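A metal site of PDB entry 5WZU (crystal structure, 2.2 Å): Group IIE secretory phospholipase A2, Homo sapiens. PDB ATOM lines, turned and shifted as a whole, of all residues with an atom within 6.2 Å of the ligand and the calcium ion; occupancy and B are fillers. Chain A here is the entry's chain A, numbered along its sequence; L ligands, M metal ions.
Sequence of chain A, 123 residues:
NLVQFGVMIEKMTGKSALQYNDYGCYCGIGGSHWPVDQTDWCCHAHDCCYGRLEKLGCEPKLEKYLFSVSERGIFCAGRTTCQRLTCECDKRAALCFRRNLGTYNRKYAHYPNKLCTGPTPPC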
ATOM      1  N   LEU A   2      14.556 -11.342   1.575  1.00  0.00           N
ATOM      2  CA  LEU A   2      15.685 -12.177   1.180  1.00  0.00           C
ATOM      3  C   LEU A   2      15.823 -13.471   2.023  1.00  0.00           C
ATOM      4  O   LEU A   2      16.923 -14.044   2.125  1.00  0.00           O
ATOM      5  CB  LEU A   2      16.954 -11.311   1.233  1.00  0.00           C
ATOM      6  CG  LEU A   2      17.968 -11.463   0.089  1.00  0.00           C
ATOM      7  CD1 LEU A   2      17.391 -11.136  -1.295  1.00  0.00           C
ATOM      8  CD2 LEU A   2      19.171 -10.579   0.404  1.00  0.00           C
ATOM      9  N   VAL A   3      14.696 -13.946   2.577  1.00  0.00           N
ATOM     10  CA  VAL A   3      14.661 -15.170   3.404  1.00  0.00           C
ATOM     11  C   VAL A   3      14.875 -16.410   2.515  1.00  0.00           C
ATOM     12  O   VAL A   3      15.709 -17.256   2.829  1.00  0.00           O
ATOM     13  CB  VAL A   3      13.334 -15.296   4.226  1.00  0.00           C
ATOM     14  CG1 VAL A   3      13.370 -16.510   5.177  1.00  0.00           C
ATOM     15  CG2 VAL A   3      13.072 -14.020   5.042  1.00  0.00           C
ATOM     16  N   PHE A   5      16.234 -16.698  -0.594  1.00  0.00           N
ATOM     17  CA  PHE A   5      17.593 -16.773  -1.235  1.00  0.00           C
ATOM     18  C   PHE A   5      18.645 -17.277  -0.248  1.00  0.00           C
ATOM     19  O   PHE A   5      19.373 -18.222  -0.543  1.00  0.00           O
ATOM     20  CB  PHE A   5      17.986 -15.422  -1.822  1.00  0.00           C
ATOM     21  CG  PHE A   5      19.274 -15.413  -2.639  1.00  0.00           C
ATOM     22  CD1 PHE A   5      19.732 -16.532  -3.346  1.00  0.00           C
ATOM     23  CD2 PHE A   5      20.012 -14.259  -2.712  1.00  0.00           C
ATOM     24  CE1 PHE A   5      20.888 -16.487  -4.093  1.00  0.00           C
ATOM     25  CE2 PHE A   5      21.178 -14.187  -3.476  1.00  0.00           C
ATOM     26  CZ  PHE A   5      21.611 -15.301  -4.165  1.00  0.00           C
ATOM     27  N   GLY A   6      18.681 -16.673   0.940  1.00  0.00           N
ATOM     28  CA  GLY A   6      19.505 -17.111   2.045  1.00  0.00           C
ATOM     29  C   GLY A   6      19.319 -18.583   2.336  1.00  0.00           C
ATOM     30  O   GLY A   6      20.284 -19.328   2.470  1.00  0.00           O
ATOM     31  N   VAL A   7      18.075 -19.039   2.387  1.00  0.00           N
ATOM     32  CA  VAL A   7      17.815 -20.446   2.642  1.00  0.00           C
ATOM     33  C   VAL A   7      18.331 -21.284   1.483  1.00  0.00           C
ATOM     34  O   VAL A   7      18.952 -22.343   1.700  1.00  0.00           O
ATOM     35  CB  VAL A   7      16.310 -20.719   2.957  1.00  0.00           C
ATOM     36  CG1 VAL A   7      15.996 -22.222   2.944  1.00  0.00           C
ATOM     37  CG2 VAL A   7      15.940 -20.095   4.294  1.00  0.00           C
ATOM     38  N   ILE A   9      20.866 -20.443  -0.591  1.00  0.00           N
ATOM     39  CA  ILE A   9      22.317 -20.407  -0.428  1.00  0.00           C
ATOM     40  C   ILE A   9      22.777 -21.454   0.610  1.00  0.00           C
ATOM     41  O   ILE A   9      23.674 -22.258   0.308  1.00  0.00           O
ATOM     42  CB  ILE A   9      22.801 -19.024  -0.002  1.00  0.00           C
ATOM     43  CG1 ILE A   9      22.674 -18.050  -1.192  1.00  0.00           C
ATOM     44  CG2 ILE A   9      24.250 -19.072   0.478  1.00  0.00           C
ATOM     45  CD1 ILE A   9      22.778 -16.602  -0.831  1.00  0.00           C
ATOM     46  N   ALA A  17      24.198 -17.927   4.886  1.00  0.00           N
ATOM     47  CA  ALA A  17      24.012 -16.844   3.893  1.00  0.00           C
ATOM     48  C   ALA A  17      24.849 -15.574   4.187  1.00  0.00           C
ATOM     49  O   ALA A  17      25.246 -14.856   3.258  1.00  0.00           O
ATOM     50  CB  ALA A  17      22.550 -16.482   3.794  1.00  0.00           C
ATOM     51  N   LEU A  18      25.099 -15.327   5.473  1.00  0.00           N
ATOM     52  CA  LEU A  18      25.964 -14.245   5.959  1.00  0.00           C
ATOM     53  C   LEU A  18      27.396 -14.309   5.378  1.00  0.00           C
ATOM     54  O   LEU A  18      28.092 -13.311   5.389  1.00  0.00           O
ATOM     55  CB  LEU A  18      26.081 -14.296   7.523  1.00  0.00           C
ATOM     56  CG  LEU A  18      24.846 -14.508   8.451  1.00  0.00           C
ATOM     57  CD1 LEU A  18      25.283 -14.768   9.894  1.00  0.00           C
ATOM     58  CD2 LEU A  18      23.844 -13.355   8.357  1.00  0.00           C
ATOM     59  N   GLN A  19      27.839 -15.493   4.969  1.00  0.00           N
ATOM     60  CA  GLN A  19      29.137 -15.678   4.361  1.00  0.00           C
ATOM     61  C   GLN A  19      29.215 -15.203   2.929  1.00  0.00           C
ATOM     62  O   GLN A  19      30.300 -15.119   2.380  1.00  0.00           O
ATOM     63  CB  GLN A  19      29.592 -17.133   4.454  1.00  0.00           C
ATOM     64  CG  GLN A  19      30.029 -17.540   5.871  1.00  0.00           C
ATOM     65  CD  GLN A  19      30.775 -18.865   5.909  1.00  0.00           C
ATOM     66  OE1 GLN A  19      30.216 -19.867   6.320  1.00  0.00           O
ATOM     67  NE2 GLN A  19      32.041 -18.866   5.481  1.00  0.00           N
ATOM     68  N   TYR A  20      28.073 -14.897   2.311  1.00  0.00           N
ATOM     69  CA  TYR A  20      28.059 -14.366   0.966  1.00  0.00           C
ATOM     70  C   TYR A  20      27.640 -12.889   0.911  1.00  0.00           C
ATOM     71  O   TYR A  20      27.670 -12.300  -0.148  1.00  0.00           O
ATOM     72  CB  TYR A  20      27.173 -15.231   0.082  1.00  0.00           C
ATOM     73  CG  TYR A  20      27.812 -16.565  -0.226  1.00  0.00           C
ATOM     74  CD1 TYR A  20      28.652 -16.728  -1.312  1.00  0.00           C
ATOM     75  CD2 TYR A  20      27.572 -17.666   0.590  1.00  0.00           C
ATOM     76  CE1 TYR A  20      29.221 -17.949  -1.599  1.00  0.00           C
ATOM     77  CE2 TYR A  20      28.150 -18.883   0.331  1.00  0.00           C
ATOM     78  CZ  TYR A  20      28.974 -19.013  -0.754  1.00  0.00           C
ATOM     79  OH  TYR A  20      29.519 -20.214  -0.993  1.00  0.00           O
ATOM     80  N   ASN A  21      27.270 -12.285   2.050  1.00  0.00           N
ATOM     81  CA  ASN A  21      27.046 -10.836   2.094  1.00  0.00           C
ATOM     82  C   ASN A  21      28.374 -10.096   2.237  1.00  0.00           C
ATOM     83  O   ASN A  21      29.285 -10.531   2.966  1.00  0.00           O
ATOM     84  CB  ASN A  21      26.152 -10.460   3.269  1.00  0.00           C
ATOM     85  CG  ASN A  21      25.705  -8.997   3.235  1.00  0.00           C
ATOM     86  OD1 ASN A  21      25.698  -8.309   4.269  1.00  0.00           O
ATOM     87  ND2 ASN A  21      25.319  -8.511   2.046  1.00  0.00           N
ATOM     88  N   ASP A  22      28.462  -8.971   1.531  1.00  0.00           N
ATOM     89  CA  ASP A  22      29.642  -8.141   1.416  1.00  0.00           C
ATOM     90  C   ASP A  22      30.839  -8.906   0.928  1.00  0.00           C
ATOM     91  O   ASP A  22      31.981  -8.385   1.029  1.00  0.00           O
ATOM     92  CB  ASP A  22      29.984  -7.452   2.728  1.00  0.00           C
ATOM     93  CG  ASP A  22      28.940  -6.531   3.149  1.00  0.00           C
ATOM     94  OD1 ASP A  22      28.405  -5.829   2.258  1.00  0.00           O
ATOM     95  OD2 ASP A  22      28.652  -6.508   4.349  1.00  0.00           O
ATOM     96  N   CYS A  25      33.331  -7.579  -4.273  1.00  0.00           N
ATOM     97  CA  CYS A  25      32.822  -6.280  -4.702  1.00  0.00           C
ATOM     98  C   CYS A  25      31.402  -6.303  -5.151  1.00  0.00           C
ATOM     99  O   CYS A  25      30.813  -5.246  -5.293  1.00  0.00           O
ATOM    100  CB  CYS A  25      33.722  -5.753  -5.823  1.00  0.00           C
ATOM    101  SG  CYS A  25      35.408  -5.536  -5.228  1.00  0.00           S
ATOM    102  N   TYR A  26      30.826  -7.498  -5.357  1.00  0.00           N
ATOM    103  CA  TYR A  26      29.485  -7.603  -5.886  1.00  0.00           C
ATOM    104  C   TYR A  26      28.439  -8.256  -4.968  1.00  0.00           C
ATOM    105  O   TYR A  26      27.240  -8.015  -5.180  1.00  0.00           O
ATOM    106  CB  TYR A  26      29.489  -8.247  -7.304  1.00  0.00           C
ATOM    107  CG  TYR A  26      29.956  -7.246  -8.329  1.00  0.00           C
ATOM    108  CD1 TYR A  26      29.051  -6.398  -8.948  1.00  0.00           C
ATOM    109  CD2 TYR A  26      31.288  -7.073  -8.566  1.00  0.00           C
ATOM    110  CE1 TYR A  26      29.481  -5.414  -9.843  1.00  0.00           C
ATOM    111  CE2 TYR A  26      31.732  -6.098  -9.444  1.00  0.00           C
ATOM    112  CZ  TYR A  26      30.834  -5.276 -10.094  1.00  0.00           C
ATOM    113  OH  TYR A  26      31.272  -4.332 -10.976  1.00  0.00           O
ATOM    114  N   CYS A  27      28.838  -9.074  -4.010  1.00  0.00           N
ATOM    115  CA  CYS A  27      27.815  -9.763  -3.242  1.00  0.00           C
ATOM    116  C   CYS A  27      27.346  -8.834  -2.119  1.00  0.00           C
ATOM    117  O   CYS A  27      28.157  -8.340  -1.317  1.00  0.00           O
ATOM    118  CB  CYS A  27      28.329 -11.074  -2.688  1.00  0.00           C
ATOM    119  SG  CYS A  27      29.095 -12.177  -3.854  1.00  0.00           S
ATOM    120  N   GLY A  28      26.048  -8.610  -2.055  1.00  0.00           N
ATOM    121  CA  GLY A  28      25.502  -7.576  -1.173  1.00  0.00           C
ATOM    122  C   GLY A  28      24.945  -6.471  -2.039  1.00  0.00           C
ATOM    123  O   GLY A  28      24.995  -6.551  -3.261  1.00  0.00           O
ATOM    124  N   ILE A  29      24.402  -5.447  -1.421  1.00  0.00           N
ATOM    125  CA  ILE A  29      23.683  -4.433  -2.214  1.00  0.00           C
ATOM    126  C   ILE A  29      24.613  -3.682  -3.180  1.00  0.00           C
ATOM    127  O   ILE A  29      25.740  -3.325  -2.833  1.00  0.00           O
ATOM    128  CB  ILE A  29      22.840  -3.457  -1.335  1.00  0.00           C
ATOM    129  CG1 ILE A  29      23.678  -2.843  -0.196  1.00  0.00           C
ATOM    130  CG2 ILE A  29      21.607  -4.199  -0.812  1.00  0.00           C
ATOM    131  CD1 ILE A  29      23.057  -1.604   0.434  1.00  0.00           C
ATOM    132  N   GLY A  30      24.143  -3.499  -4.413  1.00  0.00           N
ATOM    133  CA  GLY A  30      24.927  -2.854  -5.457  1.00  0.00           C
ATOM    134  C   GLY A  30      26.243  -3.583  -5.745  1.00  0.00           C
ATOM    135  O   GLY A  30      26.318  -4.803  -5.672  1.00  0.00           O
ATOM    136  N   GLY A  31      27.283  -2.824  -6.039  1.00  0.00           N
ATOM    137  CA  GLY A  31      28.566  -3.405  -6.449  1.00  0.00           C
ATOM    138  C   GLY A  31      29.122  -2.630  -7.615  1.00  0.00           C
ATOM    139  O   GLY A  31      28.404  -1.912  -8.279  1.00  0.00           O
ATOM    140  N   CYS A  42      29.673 -14.663  -9.706  1.00  0.00           N
ATOM    141  CA  CYS A  42      28.306 -15.117  -9.468  1.00  0.00           C
ATOM    142  C   CYS A  42      27.423 -13.963  -9.062  1.00  0.00           C
ATOM    143  O   CYS A  42      26.317 -13.847  -9.565  1.00  0.00           O
ATOM    144  CB  CYS A  42      28.191 -16.202  -8.388  1.00  0.00           C
ATOM    145  SG  CYS A  42      29.229 -17.670  -8.597  1.00  0.00           S
ATOM    146  N   CYS A  43      27.901 -13.127  -8.149  1.00  0.00           N
ATOM    147  CA  CYS A  43      27.079 -12.009  -7.663  1.00  0.00           C
ATOM    148  C   CYS A  43      26.901 -10.924  -8.702  1.00  0.00           C
ATOM    149  O   CYS A  43      25.812 -10.399  -8.844  1.00  0.00           O
ATOM    150  CB  CYS A  43      27.657 -11.434  -6.382  1.00  0.00           C
ATOM    151  SG  CYS A  43      27.548 -12.657  -5.067  1.00  0.00           S
ATOM    152  N   HIS A  44      27.960 -10.647  -9.475  1.00  0.00           N
ATOM    153  CA  HIS A  44      27.863  -9.766 -10.655  1.00  0.00           C
ATOM    154  C   HIS A  44      26.797 -10.235 -11.684  1.00  0.00           C
ATOM    155  O   HIS A  44      25.987  -9.449 -12.168  1.00  0.00           O
ATOM    156  CB  HIS A  44      29.237  -9.728 -11.344  1.00  0.00           C
ATOM    157  CG  HIS A  44      29.287  -8.859 -12.558  1.00  0.00           C
ATOM    158  ND1 HIS A  44      28.975  -9.330 -13.820  1.00  0.00           N
ATOM    159  CD2 HIS A  44      29.632  -7.569 -12.711  1.00  0.00           C
ATOM    160  CE1 HIS A  44      29.117  -8.348 -14.686  1.00  0.00           C
ATOM    161  NE2 HIS A  44      29.522  -7.269 -14.041  1.00  0.00           N
ATOM    162  N   HIS A  46      24.330 -12.202 -10.941  1.00  0.00           N
ATOM    163  CA  HIS A  46      23.057 -12.136 -10.221  1.00  0.00           C
ATOM    164  C   HIS A  46      22.483 -10.748 -10.248  1.00  0.00           C
ATOM    165  O   HIS A  46      21.277 -10.580 -10.481  1.00  0.00           O
ATOM    166  CB  HIS A  46      23.239 -12.590  -8.781  1.00  0.00           C
ATOM    167  CG  HIS A  46      21.960 -12.813  -8.027  1.00  0.00           C
ATOM    168  ND1 HIS A  46      21.533 -11.970  -7.034  1.00  0.00           N
ATOM    169  CD2 HIS A  46      21.035 -13.795  -8.103  1.00  0.00           C
ATOM    170  CE1 HIS A  46      20.390 -12.403  -6.554  1.00  0.00           C
ATOM    171  NE2 HIS A  46      20.072 -13.528  -7.168  1.00  0.00           N
ATOM    172  N   ASP A  47      23.326  -9.751  -9.999  1.00  0.00           N
ATOM    173  CA  ASP A  47      22.894  -8.364 -10.187  1.00  0.00           C
ATOM    174  C   ASP A  47      22.370  -8.081 -11.615  1.00  0.00           C
ATOM    175  O   ASP A  47      21.340  -7.419 -11.813  1.00  0.00           O
ATOM    176  CB  ASP A  47      24.069  -7.434  -9.921  1.00  0.00           C
ATOM    177  CG  ASP A  47      24.458  -7.346  -8.440  1.00  0.00           C
ATOM    178  OD1 ASP A  47      23.885  -8.048  -7.541  1.00  0.00           O
ATOM    179  OD2 ASP A  47      25.374  -6.541  -8.192  1.00  0.00           O
ATOM    180  N   TYR A  50      18.932  -9.608 -11.940  1.00  0.00           N
ATOM    181  CA  TYR A  50      17.896  -8.773 -11.343  1.00  0.00           C
ATOM    182  C   TYR A  50      17.565  -7.531 -12.202  1.00  0.00           C
ATOM    183  O   TYR A  50      16.397  -7.165 -12.311  1.00  0.00           O
ATOM    184  CB  TYR A  50      18.258  -8.351  -9.890  1.00  0.00           C
ATOM    185  CG  TYR A  50      17.884  -9.348  -8.769  1.00  0.00           C
ATOM    186  CD1 TYR A  50      17.678 -10.706  -9.023  1.00  0.00           C
ATOM    187  CD2 TYR A  50      17.724  -8.922  -7.434  1.00  0.00           C
ATOM    188  CE1 TYR A  50      17.302 -11.587  -8.009  1.00  0.00           C
ATOM    189  CE2 TYR A  50      17.349  -9.811  -6.409  1.00  0.00           C
ATOM    190  CZ  TYR A  50      17.183 -11.138  -6.691  1.00  0.00           C
ATOM    191  OH  TYR A  50      16.818 -12.034  -5.699  1.00  0.00           O
ATOM    192  N   LYS A  61      13.923  -7.767  -5.941  1.00  0.00           N
ATOM    193  CA  LYS A  61      14.361  -7.527  -4.556  1.00  0.00           C
ATOM    194  C   LYS A  61      13.274  -7.825  -3.549  1.00  0.00           C
ATOM    195  O   LYS A  61      13.570  -8.082  -2.400  1.00  0.00           O
ATOM    196  CB  LYS A  61      14.864  -6.092  -4.375  1.00  0.00           C
ATOM    197  CG  LYS A  61      16.236  -5.879  -4.988  1.00  0.00           C
ATOM    198  CD  LYS A  61      16.611  -4.423  -5.169  1.00  0.00           C
ATOM    199  CE  LYS A  61      18.126  -4.277  -5.103  1.00  0.00           C
ATOM    200  NZ  LYS A  61      18.598  -2.984  -5.677  1.00  0.00           N
ATOM    201  N   ALA A  93      22.570 -18.315  -9.244  1.00  0.00           N
ATOM    202  CA  ALA A  93      23.560 -17.825  -8.266  1.00  0.00           C
ATOM    203  C   ALA A  93      23.975 -18.860  -7.246  1.00  0.00           C
ATOM    204  O   ALA A  93      25.173 -19.035  -6.999  1.00  0.00           O
ATOM    205  CB  ALA A  93      23.066 -16.553  -7.586  1.00  0.00           C
ATOM    206  N   PHE A  97      27.611 -20.403  -6.729  1.00  0.00           N
ATOM    207  CA  PHE A  97      28.341 -20.475  -5.434  1.00  0.00           C
ATOM    208  C   PHE A  97      28.852 -21.892  -5.110  1.00  0.00           C
ATOM    209  O   PHE A  97      30.052 -22.086  -4.850  1.00  0.00           O
ATOM    210  CB  PHE A  97      27.508 -20.013  -4.247  1.00  0.00           C
ATOM    211  CG  PHE A  97      27.051 -18.581  -4.295  1.00  0.00           C
ATOM    212  CD1 PHE A  97      27.784 -17.565  -4.942  1.00  0.00           C
ATOM    213  CD2 PHE A  97      25.890 -18.218  -3.614  1.00  0.00           C
ATOM    214  CE1 PHE A  97      27.338 -16.247  -4.928  1.00  0.00           C
ATOM    215  CE2 PHE A  97      25.441 -16.901  -3.609  1.00  0.00           C
ATOM    216  CZ  PHE A  97      26.181 -15.906  -4.256  1.00  0.00           C
HETATM  217  O1  LIG L   1      20.675  -6.669  -6.528  1.00  0.00           O
HETATM  218  C1  LIG L   1      21.317  -6.952  -5.477  1.00  0.00           C
HETATM  219  O2  LIG L   1      22.286  -6.274  -5.020  1.00  0.00           O
HETATM  220  C2  LIG L   1      20.884  -8.221  -4.717  1.00  0.00           C
HETATM  221  O3  LIG L   1      22.063  -8.745  -4.033  1.00  0.00           O
HETATM  222  C3  LIG L   1      22.117  -9.002  -2.668  1.00  0.00           C
HETATM  223  C4  LIG L   1      21.519  -8.085  -1.788  1.00  0.00           C
HETATM  224  C5  LIG L   1      21.577  -8.312  -0.428  1.00  0.00           C
HETATM  225  C6  LIG L   1      22.264  -9.437   0.008  1.00  0.00           C
HETATM  226  C7  LIG L   1      22.844 -10.309  -0.851  1.00  0.00           C
HETATM  227  C8  LIG L   1      22.795 -10.121  -2.199  1.00  0.00           C
HETATM  228  C9  LIG L   1      23.495 -11.172  -2.738  1.00  0.00           C
HETATM  229  C10 LIG L   1      23.764 -11.442  -4.040  1.00  0.00           C
HETATM  230  O4  LIG L   1      23.538 -12.527  -4.583  1.00  0.00           O
HETATM  231  C11 LIG L   1      24.420 -10.335  -4.885  1.00  0.00           C
HETATM  232  O5  LIG L   1      24.725  -9.248  -4.399  1.00  0.00           O
HETATM  233  N1  LIG L   1      24.561 -10.587  -6.169  1.00  0.00           N
HETATM  234  C12 LIG L   1      23.914 -11.945  -1.738  1.00  0.00           C
HETATM  235  C13 LIG L   1      24.731 -13.233  -1.939  1.00  0.00           C
HETATM  236  N2  LIG L   1      23.517 -11.435  -0.569  1.00  0.00           N
HETATM  237  C14 LIG L   1      23.736 -11.952   0.888  1.00  0.00           C
HETATM  238  C15 LIG L   1      22.534 -12.528   1.457  1.00  0.00           C
HETATM  239  C16 LIG L   1      21.780 -13.343   0.598  1.00  0.00           C
HETATM  240  C17 LIG L   1      20.597 -13.956   1.007  1.00  0.00           C
HETATM  241  C18 LIG L   1      20.137 -13.797   2.299  1.00  0.00           C
HETATM  242  C19 LIG L   1      20.848 -13.014   3.175  1.00  0.00           C
HETATM  243  C20 LIG L   1      22.051 -12.357   2.808  1.00  0.00           C
HETATM  244  C21 LIG L   1      22.676 -11.575   3.817  1.00  0.00           C
HETATM  245  F1  LIG L   1      21.883 -11.401   5.014  1.00  0.00           F
HETATM  246  F2  LIG L   1      22.910 -10.324   3.388  1.00  0.00           F
HETATM  247  F3  LIG L   1      23.874 -12.231   4.183  1.00  0.00           F
HETATM  248 CA    CA M   1      25.362  -7.020  -5.460  1.00  0.00          CA
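N of Gly 28 lies close to O5 of the ligand (2.8 Å). N of Gly 30 lies within hydrogen-bond range of O2 of the ligand (3.4 Å). The backbone carbonyl oxygen (O) of Cys 43 lies within hydrogen-bond range of a nitrogen (N1) of the ligand. N1 of the ligand sits close to SG of Cys 43, at 3.8 Å. A ring nitrogen (ND1) of His 46 is in hydrogen-bond range of an oxygen (O4) of the ligand, 3.2 Å away.
SG of Cys 43 forms a disulfide with SG of Cys 27, at 2.0 Å. The side-chain carboxylate (OD2) of Asp 22 sits close to the side-chain amide oxygen (OD1) of Asn 21 (3.5 Å). N of Asp 22 lies within hydrogen-bond range of O of Cys 27. N of Phe 97 lies within hydrogen-bond range of SG of Cys 42.
A fluorine (F3) of the ligand sits close to the backbone carbonyl oxygen of Ala 17, at 3.1 Å. ND2 of Asn 21 sits close to F2 of the ligand (3.3 Å). Merely in contact with the ligand: Leu 2 (3.2 Å), Phe 5 (3.1 Å), Gly 6 (3.3 Å), Ile 9 (3.7 Å), Leu 18 (3.4 Å), Tyr 20 (3.6 Å), Cys 27 (3.3 Å), Ile 29 (3.6 Å), Tyr 50 (3.8 Å), Lys 61 (3.8 Å) and Phe 97 (3.8 Å). Hydrophobic or aromatic side chains within 4 Å of the ligand: Leu 2, Phe 5, Ile 9, Ala 17, Tyr 20, His 46, Tyr 50 and Phe 97. 19 residues have an atom within 4 Å of the ligand: Leu 2, Phe 5, Gly 6, Ile 9, Ala 17, Leu 18, Tyr 20, Asn 21, Tyr 26, Cys 27, Gly 28, Ile 29, Gly 30, Cys 43, His 46, Asp 47, Tyr 50, Lys 61 and Phe 97. The nearest printed residue that does not touch the ligand is His 44 (4.7 Å).
Of the 28 residues printed, 4 come within 4 Å of the calcium ion. The nearest printed residue that does not touch the calcium ion is Ile 29 (4.1 Å).
The calcium ion is bound by the backbone carbonyl oxygen (O) of Tyr 26 (2.1 Å), the backbone carbonyl oxygen (O) of Gly 28 (2.3 Å), the backbone carbonyl oxygen (O) of Gly 30 (2.4 Å), an oxygen (O5) of the ligand (2.5 Å), the side-chain carboxylate (OD1) of Asp 47 (2.8 Å) and the side-chain carboxylate (OD2) of Asp 47 (2.8 Å).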
